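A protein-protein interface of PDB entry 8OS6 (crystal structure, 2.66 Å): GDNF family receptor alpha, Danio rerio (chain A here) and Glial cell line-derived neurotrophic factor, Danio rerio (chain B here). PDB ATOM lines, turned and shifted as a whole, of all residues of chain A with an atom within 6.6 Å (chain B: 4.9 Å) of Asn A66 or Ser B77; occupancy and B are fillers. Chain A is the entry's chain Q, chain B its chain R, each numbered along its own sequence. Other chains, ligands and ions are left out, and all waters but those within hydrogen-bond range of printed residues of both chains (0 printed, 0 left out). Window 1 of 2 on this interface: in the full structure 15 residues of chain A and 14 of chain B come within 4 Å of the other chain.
Cys A65 touches none of the printed residues of chain B.
Printed residues of chain B within 4 Å of Leu A67: Glu B27.
Lys A73 touches none of the printed residues of chain B.
Of the printed residues of chain B, Ile A79 touches Ser B77 (3.6 Å) and Thr B87 (3.6 Å).
Of the printed residues of chain A, Glu B27 touches Lys A63, Asn A66 and Leu A67.
Ser B77 touches just these residues of chain A: Asn A66, Arg A75, Ser A76 and Ile A79.
Of the printed residues of chain A, Thr B87 touches Ser A76, Ile A79 and Ser A80.
The nearest residue of chain A that does not touch Ser B77 is Ser A80 (4.6 Å).
Of the 19 printed residues of chain A, 9 touch a printed residue of chain B.
Among the printed residues, Asp or Glu carboxylates within 4 Å of a Lys or Arg side-chain nitrogen of the other chain: Lys A63 with Glu B27 and Arg A75 with Glu B26.
Among the printed residues, pairs that only touch across the chains: Ser A76 with Asp B75 (3.5 Å), Ser A80 with Thr B87 (3.5 Å), Ser A76 with Ile B76 (3.6 Å), Ile A79 with Ser B77 (3.6 Å), Ile A79 with Thr B87 (3.6 Å), Lys A72 with Ile B76 (3.7 Å), Ser A76 with Thr B87 (3.7 Å), Arg A75 with Ser B77 (3.9 Å), Ala A62 with Glu B26 (3.9 Å), Leu A67 with Glu B27 (3.98 Å) and Asn A66 with Ile B76 (3.99 Å).
NZ of Lys A63 is in salt-bridge range of OE2 of Glu B27, at 3.7 Å.
OE1 of Glu B26 sits at hydrogen-bond distance from ND2 of Asn A66, at 3.0 Å.
O of Glu B27 lies within hydrogen-bond range of ND2 of Asn A66 (3.3 Å).
The side-chain amide nitrogen (ND2) of Asn A66 lies within hydrogen-bond range of the backbone carbonyl oxygen (O) of Ser B77.
The backbone carbonyl oxygen of Asp B75 sits close to the side-chain amino group of Lys A72, 3.4 Å away.
NH2 of Arg A75 lies within salt-bridge range of OE2 of Glu B26.
OG of Ser A76 is in hydrogen-bond range of OG of Ser B77.
N of Lys A72 sits at hydrogen-bond distance from O of Cys A65.
OD1 of Asn A66 lies within hydrogen-bond range of NH1 of Arg A75.
The backbone carbonyl oxygen (O) of Ser A76 is in hydrogen-bond range of the side-chain hydroxyl (OG) of Ser A80 (3.3 Å).
The side-chain carboxylate (OE2) of Glu B26 is in hydrogen-bond range of the backbone NH (N) of Leu B79, at 3.4 Å.
OG1 of Thr B87 lies within hydrogen-bond range of OG of Ser B77 (2.9 Å).
The side-chain sulfur (SG) of Cys A65 forms a disulfide with the side-chain sulfur (SG) of Cys A71 (2.0 Å).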
ATOM      1  N   ALA A  61      -2.128  11.622   2.052  1.00  0.00           N
ATOM      2  CA  ALA A  61      -1.233  11.639   3.204  1.00  0.00           C
ATOM      3  C   ALA A  61       0.165  11.171   2.821  1.00  0.00           C
ATOM      4  O   ALA A  61       1.164  11.727   3.292  1.00  0.00           O
ATOM      5  CB  ALA A  61      -1.801  10.767   4.322  1.00  0.00           C
ATOM      6  N   ALA A  62       0.256  10.145   1.970  1.00  0.00           N
ATOM      7  CA  ALA A  62       1.562   9.671   1.523  1.00  0.00           C
ATOM      8  C   ALA A  62       2.311  10.759   0.763  1.00  0.00           C
ATOM      9  O   ALA A  62       3.515  10.954   0.967  1.00  0.00           O
ATOM     10  CB  ALA A  62       1.396   8.426   0.653  1.00  0.00           C
ATOM     11  N   LYS A  63       1.615  11.477  -0.121  1.00  0.00           N
ATOM     12  CA  LYS A  63       2.252  12.565  -0.855  1.00  0.00           C
ATOM     13  C   LYS A  63       2.834  13.601   0.099  1.00  0.00           C
ATOM     14  O   LYS A  63       3.974  14.048  -0.070  1.00  0.00           O
ATOM     15  CB  LYS A  63       1.244  13.213  -1.803  1.00  0.00           C
ATOM     16  CG  LYS A  63       0.799  12.315  -2.942  1.00  0.00           C
ATOM     17  CD  LYS A  63      -0.393  12.911  -3.676  1.00  0.00           C
ATOM     18  CE  LYS A  63      -0.774  12.083  -4.895  1.00  0.00           C
ATOM     19  NZ  LYS A  63      -2.088  12.502  -5.465  1.00  0.00           N
ATOM     20  N   ALA A  64       2.060  13.995   1.111  1.00  0.00           N
ATOM     21  CA  ALA A  64       2.549  14.983   2.067  1.00  0.00           C
ATOM     22  C   ALA A  64       3.814  14.505   2.767  1.00  0.00           C
ATOM     23  O   ALA A  64       4.689  15.318   3.089  1.00  0.00           O
ATOM     24  CB  ALA A  64       1.465  15.299   3.097  1.00  0.00           C
ATOM     25  N   CYS A  65       3.935  13.197   3.005  1.00  0.00           N
ATOM     26  CA  CYS A  65       5.112  12.678   3.694  1.00  0.00           C
ATOM     27  C   CYS A  65       6.343  12.717   2.796  1.00  0.00           C
ATOM     28  O   CYS A  65       7.439  13.061   3.253  1.00  0.00           O
ATOM     29  CB  CYS A  65       4.840  11.256   4.180  1.00  0.00           C
ATOM     30  SG  CYS A  65       6.226  10.447   5.016  1.00  0.00           S
ATOM     31  N   ASN A  66       6.183  12.377   1.514  1.00  0.00           N
ATOM     32  CA  ASN A  66       7.323  12.394   0.603  1.00  0.00           C
ATOM     33  C   ASN A  66       7.838  13.809   0.366  1.00  0.00           C
ATOM     34  O   ASN A  66       9.040  13.999   0.146  1.00  0.00           O
ATOM     35  CB  ASN A  66       6.945  11.744  -0.728  1.00  0.00           C
ATOM     36  CG  ASN A  66       7.221  10.252  -0.751  1.00  0.00           C
ATOM     37  OD1 ASN A  66       7.601   9.659   0.260  1.00  0.00           O
ATOM     38  ND2 ASN A  66       7.028   9.636  -1.911  1.00  0.00           N
ATOM     39  N   LEU A  67       6.957  14.804   0.402  1.00  0.00           N
ATOM     40  CA  LEU A  67       7.346  16.192   0.193  1.00  0.00           C
ATOM     41  C   LEU A  67       7.828  16.870   1.469  1.00  0.00           C
ATOM     42  O   LEU A  67       8.193  18.049   1.426  1.00  0.00           O
ATOM     43  CB  LEU A  67       6.176  16.981  -0.398  1.00  0.00           C
ATOM     44  CG  LEU A  67       6.043  16.906  -1.920  1.00  0.00           C
ATOM     45  CD1 LEU A  67       6.221  15.481  -2.423  1.00  0.00           C
ATOM     46  CD2 LEU A  67       4.697  17.464  -2.361  1.00  0.00           C
ATOM     47  N   ASN A  68       7.833  16.161   2.592  1.00  0.00           N
ATOM     48  CA  ASN A  68       8.399  16.649   3.843  1.00  0.00           C
ATOM     49  C   ASN A  68       9.710  15.910   4.080  1.00  0.00           C
ATOM     50  O   ASN A  68       9.713  14.686   4.247  1.00  0.00           O
ATOM     51  CB  ASN A  68       7.428  16.433   5.003  1.00  0.00           C
ATOM     52  CG  ASN A  68       7.883  17.111   6.277  1.00  0.00           C
ATOM     53  OD1 ASN A  68       8.406  16.465   7.185  1.00  0.00           O
ATOM     54  ND2 ASN A  68       7.689  18.424   6.350  1.00  0.00           N
ATOM     55  N   ASP A  69      10.818  16.657   4.092  1.00  0.00           N
ATOM     56  CA  ASP A  69      12.138  16.032   4.111  1.00  0.00           C
ATOM     57  C   ASP A  69      12.263  15.007   5.231  1.00  0.00           C
ATOM     58  O   ASP A  69      12.759  13.895   5.016  1.00  0.00           O
ATOM     59  CB  ASP A  69      13.221  17.106   4.241  1.00  0.00           C
ATOM     60  CG  ASP A  69      13.398  17.914   2.969  1.00  0.00           C
ATOM     61  OD1 ASP A  69      12.547  17.787   2.063  1.00  0.00           O
ATOM     62  OD2 ASP A  69      14.391  18.668   2.870  1.00  0.00           O
ATOM     63  N   CYS A  71       9.867  13.364   7.030  1.00  0.00           N
ATOM     64  CA  CYS A  71       8.997  12.201   6.884  1.00  0.00           C
ATOM     65  C   CYS A  71       9.457  11.313   5.733  1.00  0.00           C
ATOM     66  O   CYS A  71       9.406  10.081   5.833  1.00  0.00           O
ATOM     67  CB  CYS A  71       7.548  12.646   6.675  1.00  0.00           C
ATOM     68  SG  CYS A  71       6.318  11.319   6.850  1.00  0.00           S
ATOM     69  N   LYS A  72       9.918  11.918   4.636  1.00  0.00           N
ATOM     70  CA  LYS A  72      10.396  11.128   3.505  1.00  0.00           C
ATOM     71  C   LYS A  72      11.629  10.321   3.887  1.00  0.00           C
ATOM     72  O   LYS A  72      11.749   9.145   3.525  1.00  0.00           O
ATOM     73  CB  LYS A  72      10.701  12.041   2.317  1.00  0.00           C
ATOM     74  CG  LYS A  72      10.934  11.303   1.006  1.00  0.00           C
ATOM     75  CD  LYS A  72      12.410  11.036   0.745  1.00  0.00           C
ATOM     76  CE  LYS A  72      13.135  12.285   0.263  1.00  0.00           C
ATOM     77  NZ  LYS A  72      14.537  11.991  -0.157  1.00  0.00           N
ATOM     78  N   LYS A  73      12.557  10.940   4.620  1.00  0.00           N
ATOM     79  CA  LYS A  73      13.775  10.244   5.024  1.00  0.00           C
ATOM     80  C   LYS A  73      13.452   9.021   5.872  1.00  0.00           C
ATOM     81  O   LYS A  73      13.934   7.915   5.598  1.00  0.00           O
ATOM     82  CB  LYS A  73      14.689  11.207   5.786  1.00  0.00           C
ATOM     83  CG  LYS A  73      15.940  10.565   6.364  1.00  0.00           C
ATOM     84  CD  LYS A  73      16.807  11.592   7.083  1.00  0.00           C
ATOM     85  CE  LYS A  73      17.974  10.928   7.801  1.00  0.00           C
ATOM     86  NZ  LYS A  73      18.851  11.920   8.485  1.00  0.00           N
ATOM     87  N   ARG A  75      10.468   7.531   6.349  1.00  0.00           N
ATOM     88  CA  ARG A  75       9.613   6.567   5.667  1.00  0.00           C
ATOM     89  C   ARG A  75      10.457   5.569   4.884  1.00  0.00           C
ATOM     90  O   ARG A  75      10.211   4.359   4.932  1.00  0.00           O
ATOM     91  CB  ARG A  75       8.628   7.277   4.739  1.00  0.00           C
ATOM     92  CG  ARG A  75       7.605   6.333   4.114  1.00  0.00           C
ATOM     93  CD  ARG A  75       6.793   6.996   3.011  1.00  0.00           C
ATOM     94  NE  ARG A  75       5.967   6.024   2.303  1.00  0.00           N
ATOM     95  CZ  ARG A  75       5.225   6.296   1.239  1.00  0.00           C
ATOM     96  NH1 ARG A  75       5.177   7.514   0.722  1.00  0.00           N
ATOM     97  NH2 ARG A  75       4.516   5.322   0.675  1.00  0.00           N
ATOM     98  N   SER A  76      11.472   6.062   4.168  1.00  0.00           N
ATOM     99  CA  SER A  76      12.386   5.169   3.467  1.00  0.00           C
ATOM    100  C   SER A  76      13.216   4.346   4.441  1.00  0.00           C
ATOM    101  O   SER A  76      13.656   3.241   4.102  1.00  0.00           O
ATOM    102  CB  SER A  76      13.301   5.981   2.548  1.00  0.00           C
ATOM    103  OG  SER A  76      13.631   5.258   1.376  1.00  0.00           O
ATOM    104  N   ALA A  77      13.430   4.856   5.656  1.00  0.00           N
ATOM    105  CA  ALA A  77      14.265   4.148   6.618  1.00  0.00           C
ATOM    106  C   ALA A  77      13.648   2.822   7.044  1.00  0.00           C
ATOM    107  O   ALA A  77      14.383   1.885   7.375  1.00  0.00           O
ATOM    108  CB  ALA A  77      14.516   5.024   7.845  1.00  0.00           C
ATOM    109  N   ILE A  79      10.932   1.333   5.095  1.00  0.00           N
ATOM    110  CA  ILE A  79      10.509   0.589   3.912  1.00  0.00           C
ATOM    111  C   ILE A  79      11.637  -0.312   3.422  1.00  0.00           C
ATOM    112  O   ILE A  79      11.400  -1.434   2.962  1.00  0.00           O
ATOM    113  CB  ILE A  79      10.041   1.556   2.809  1.00  0.00           C
ATOM    114  CG1 ILE A  79       8.704   2.203   3.182  1.00  0.00           C
ATOM    115  CG2 ILE A  79       9.926   0.829   1.475  1.00  0.00           C
ATOM    116  CD1 ILE A  79       7.537   1.234   3.261  1.00  0.00           C
ATOM    117  N   SER A  80      12.887   0.162   3.522  1.00  0.00           N
ATOM    118  CA  SER A  80      14.007  -0.622   3.002  1.00  0.00           C
ATOM    119  C   SER A  80      14.244  -1.881   3.826  1.00  0.00           C
ATOM    120  O   SER A  80      14.198  -2.990   3.262  1.00  0.00           O
ATOM    121  CB  SER A  80      15.260   0.252   2.920  1.00  0.00           C
ATOM    122  OG  SER A  80      15.109   1.264   1.938  1.00  0.00           O
ATOM    123  N   HIS A 112       2.234  14.126  10.131  1.00  0.00           N
ATOM    124  CA  HIS A 112       2.524  13.317   8.952  1.00  0.00           C
ATOM    125  C   HIS A 112       2.484  11.820   9.246  1.00  0.00           C
ATOM    126  O   HIS A 112       1.904  11.050   8.473  1.00  0.00           O
ATOM    127  CB  HIS A 112       3.900  13.688   8.381  1.00  0.00           C
ATOM    128  CG  HIS A 112       3.958  15.053   7.770  1.00  0.00           C
ATOM    129  ND1 HIS A 112       4.457  16.150   8.440  1.00  0.00           N
ATOM    130  CD2 HIS A 112       3.586  15.499   6.547  1.00  0.00           C
ATOM    131  CE1 HIS A 112       4.387  17.212   7.658  1.00  0.00           C
ATOM    132  NE2 HIS A 112       3.860  16.844   6.504  1.00  0.00           N
ATOM    133  N   MET A 116      -0.876   9.082   8.088  1.00  0.00           N
ATOM    134  CA  MET A 116      -0.825   7.923   7.208  1.00  0.00           C
ATOM    135  C   MET A 116      -1.429   6.682   7.855  1.00  0.00           C
ATOM    136  O   MET A 116      -2.170   5.941   7.200  1.00  0.00           O
ATOM    137  CB  MET A 116       0.624   7.637   6.798  1.00  0.00           C
ATOM    138  CG  MET A 116       1.251   8.709   5.914  1.00  0.00           C
ATOM    139  SD  MET A 116       2.998   8.419   5.555  1.00  0.00           S
ATOM    140  CE  MET A 116       2.895   7.158   4.286  1.00  0.00           C
ATOM    141  N   GLU B  26       2.221   8.552  -6.647  1.00  0.00           N
ATOM    142  CA  GLU B  26       3.015   9.268  -5.662  1.00  0.00           C
ATOM    143  C   GLU B  26       3.719  10.458  -6.312  1.00  0.00           C
ATOM    144  O   GLU B  26       3.775  10.595  -7.538  1.00  0.00           O
ATOM    145  CB  GLU B  26       4.037   8.333  -5.015  1.00  0.00           C
ATOM    146  CG  GLU B  26       3.436   7.321  -4.048  1.00  0.00           C
ATOM    147  CD  GLU B  26       3.849   7.564  -2.605  1.00  0.00           C
ATOM    148  OE1 GLU B  26       4.197   8.714  -2.261  1.00  0.00           O
ATOM    149  OE2 GLU B  26       3.828   6.597  -1.813  1.00  0.00           O
ATOM    150  N   GLU B  27       4.264  11.329  -5.465  1.00  0.00           N
ATOM    151  CA  GLU B  27       4.927  12.547  -5.907  1.00  0.00           C
ATOM    152  C   GLU B  27       6.297  12.648  -5.250  1.00  0.00           C
ATOM    153  O   GLU B  27       6.608  11.935  -4.290  1.00  0.00           O
ATOM    154  CB  GLU B  27       4.077  13.784  -5.584  1.00  0.00           C
ATOM    155  CG  GLU B  27       2.707  13.780  -6.247  1.00  0.00           C
ATOM    156  CD  GLU B  27       1.847  14.945  -5.802  1.00  0.00           C
ATOM    157  OE1 GLU B  27       2.400  15.892  -5.204  1.00  0.00           O
ATOM    158  OE2 GLU B  27       0.620  14.913  -6.043  1.00  0.00           O
ATOM    159  N   ASP B  75      17.242   8.812   0.599  1.00  0.00           N
ATOM    160  CA  ASP B  75      16.497   7.859  -0.206  1.00  0.00           C
ATOM    161  C   ASP B  75      15.000   8.152  -0.143  1.00  0.00           C
ATOM    162  O   ASP B  75      14.496   8.763   0.803  1.00  0.00           O
ATOM    163  CB  ASP B  75      16.773   6.434   0.269  1.00  0.00           C
ATOM    164  CG  ASP B  75      18.253   6.156   0.446  1.00  0.00           C
ATOM    165  OD1 ASP B  75      19.050   6.615  -0.401  1.00  0.00           O
ATOM    166  OD2 ASP B  75      18.622   5.488   1.436  1.00  0.00           O
ATOM    167  N   ILE B  76      14.287   7.698  -1.171  1.00  0.00           N
ATOM    168  CA  ILE B  76      12.850   7.909  -1.290  1.00  0.00           C
ATOM    169  C   ILE B  76      12.189   6.585  -1.644  1.00  0.00           C
ATOM    170  O   ILE B  76      12.674   5.849  -2.511  1.00  0.00           O
ATOM    171  CB  ILE B  76      12.521   8.985  -2.346  1.00  0.00           C
ATOM    172  CG1 ILE B  76      11.055   9.408  -2.235  1.00  0.00           C
ATOM    173  CG2 ILE B  76      12.809   8.463  -3.747  1.00  0.00           C
ATOM    174  CD1 ILE B  76      10.717  10.650  -3.031  1.00  0.00           C
ATOM    175  N   SER B  77      11.079   6.286  -0.971  1.00  0.00           N
ATOM    176  CA  SER B  77      10.308   5.075  -1.202  1.00  0.00           C
ATOM    177  C   SER B  77       8.877   5.444  -1.566  1.00  0.00           C
ATOM    178  O   SER B  77       8.383   6.513  -1.194  1.00  0.00           O
ATOM    179  CB  SER B  77      10.308   4.167   0.033  1.00  0.00           C
ATOM    180  OG  SER B  77      11.627   3.799   0.396  1.00  0.00           O
ATOM    181  N   PHE B  78       8.212   4.549  -2.293  1.00  0.00           N
ATOM    182  CA  PHE B  78       6.836   4.784  -2.702  1.00  0.00           C
ATOM    183  C   PHE B  78       6.134   3.451  -2.924  1.00  0.00           C
ATOM    184  O   PHE B  78       6.772   2.404  -3.059  1.00  0.00           O
ATOM    185  CB  PHE B  78       6.770   5.643  -3.971  1.00  0.00           C
ATOM    186  CG  PHE B  78       7.595   5.112  -5.106  1.00  0.00           C
ATOM    187  CD1 PHE B  78       7.050   4.232  -6.024  1.00  0.00           C
ATOM    188  CD2 PHE B  78       8.913   5.497  -5.258  1.00  0.00           C
ATOM    189  CE1 PHE B  78       7.807   3.744  -7.071  1.00  0.00           C
ATOM    190  CE2 PHE B  78       9.675   5.013  -6.301  1.00  0.00           C
ATOM    191  CZ  PHE B  78       9.121   4.135  -7.209  1.00  0.00           C
ATOM    192  N   LEU B  79       4.804   3.510  -2.958  1.00  0.00           N
ATOM    193  CA  LEU B  79       3.955   2.343  -3.159  1.00  0.00           C
ATOM    194  C   LEU B  79       3.265   2.442  -4.512  1.00  0.00           C
ATOM    195  O   LEU B  79       2.735   3.501  -4.868  1.00  0.00           O
ATOM    196  CB  LEU B  79       2.910   2.232  -2.049  1.00  0.00           C
ATOM    197  CG  LEU B  79       2.068   0.956  -2.041  1.00  0.00           C
ATOM    198  CD1 LEU B  79       2.918  -0.240  -1.636  1.00  0.00           C
ATOM    199  CD2 LEU B  79       0.869   1.109  -1.116  1.00  0.00           C
ATOM    200  N   HIS B  86       8.707   0.148  -3.552  1.00  0.00           N
ATOM    201  CA  HIS B  86       9.915   0.398  -4.324  1.00  0.00           C
ATOM    202  C   HIS B  86      10.707   1.515  -3.664  1.00  0.00           C
ATOM    203  O   HIS B  86      10.129   2.487  -3.169  1.00  0.00           O
ATOM    204  CB  HIS B  86       9.584   0.771  -5.773  1.00  0.00           C
ATOM    205  CG  HIS B  86       8.892  -0.316  -6.534  1.00  0.00           C
ATOM    206  ND1 HIS B  86       9.537  -1.463  -6.944  1.00  0.00           N
ATOM    207  CD2 HIS B  86       7.613  -0.430  -6.963  1.00  0.00           C
ATOM    208  CE1 HIS B  86       8.684  -2.238  -7.591  1.00  0.00           C
ATOM    209  NE2 HIS B  86       7.510  -1.634  -7.617  1.00  0.00           N
ATOM    210  N   THR B  87      12.031   1.371  -3.660  1.00  0.00           N
ATOM    211  CA  THR B  87      12.929   2.342  -3.050  1.00  0.00           C
ATOM    212  C   THR B  87      13.978   2.760  -4.068  1.00  0.00           C
ATOM    213  O   THR B  87      14.574   1.909  -4.737  1.00  0.00           O
ATOM    214  CB  THR B  87      13.610   1.765  -1.804  1.00  0.00           C
ATOM    215  OG1 THR B  87      12.616   1.377  -0.849  1.00  0.00           O
ATOM    216  CG2 THR B  87      14.539   2.792  -1.172  1.00  0.00           C
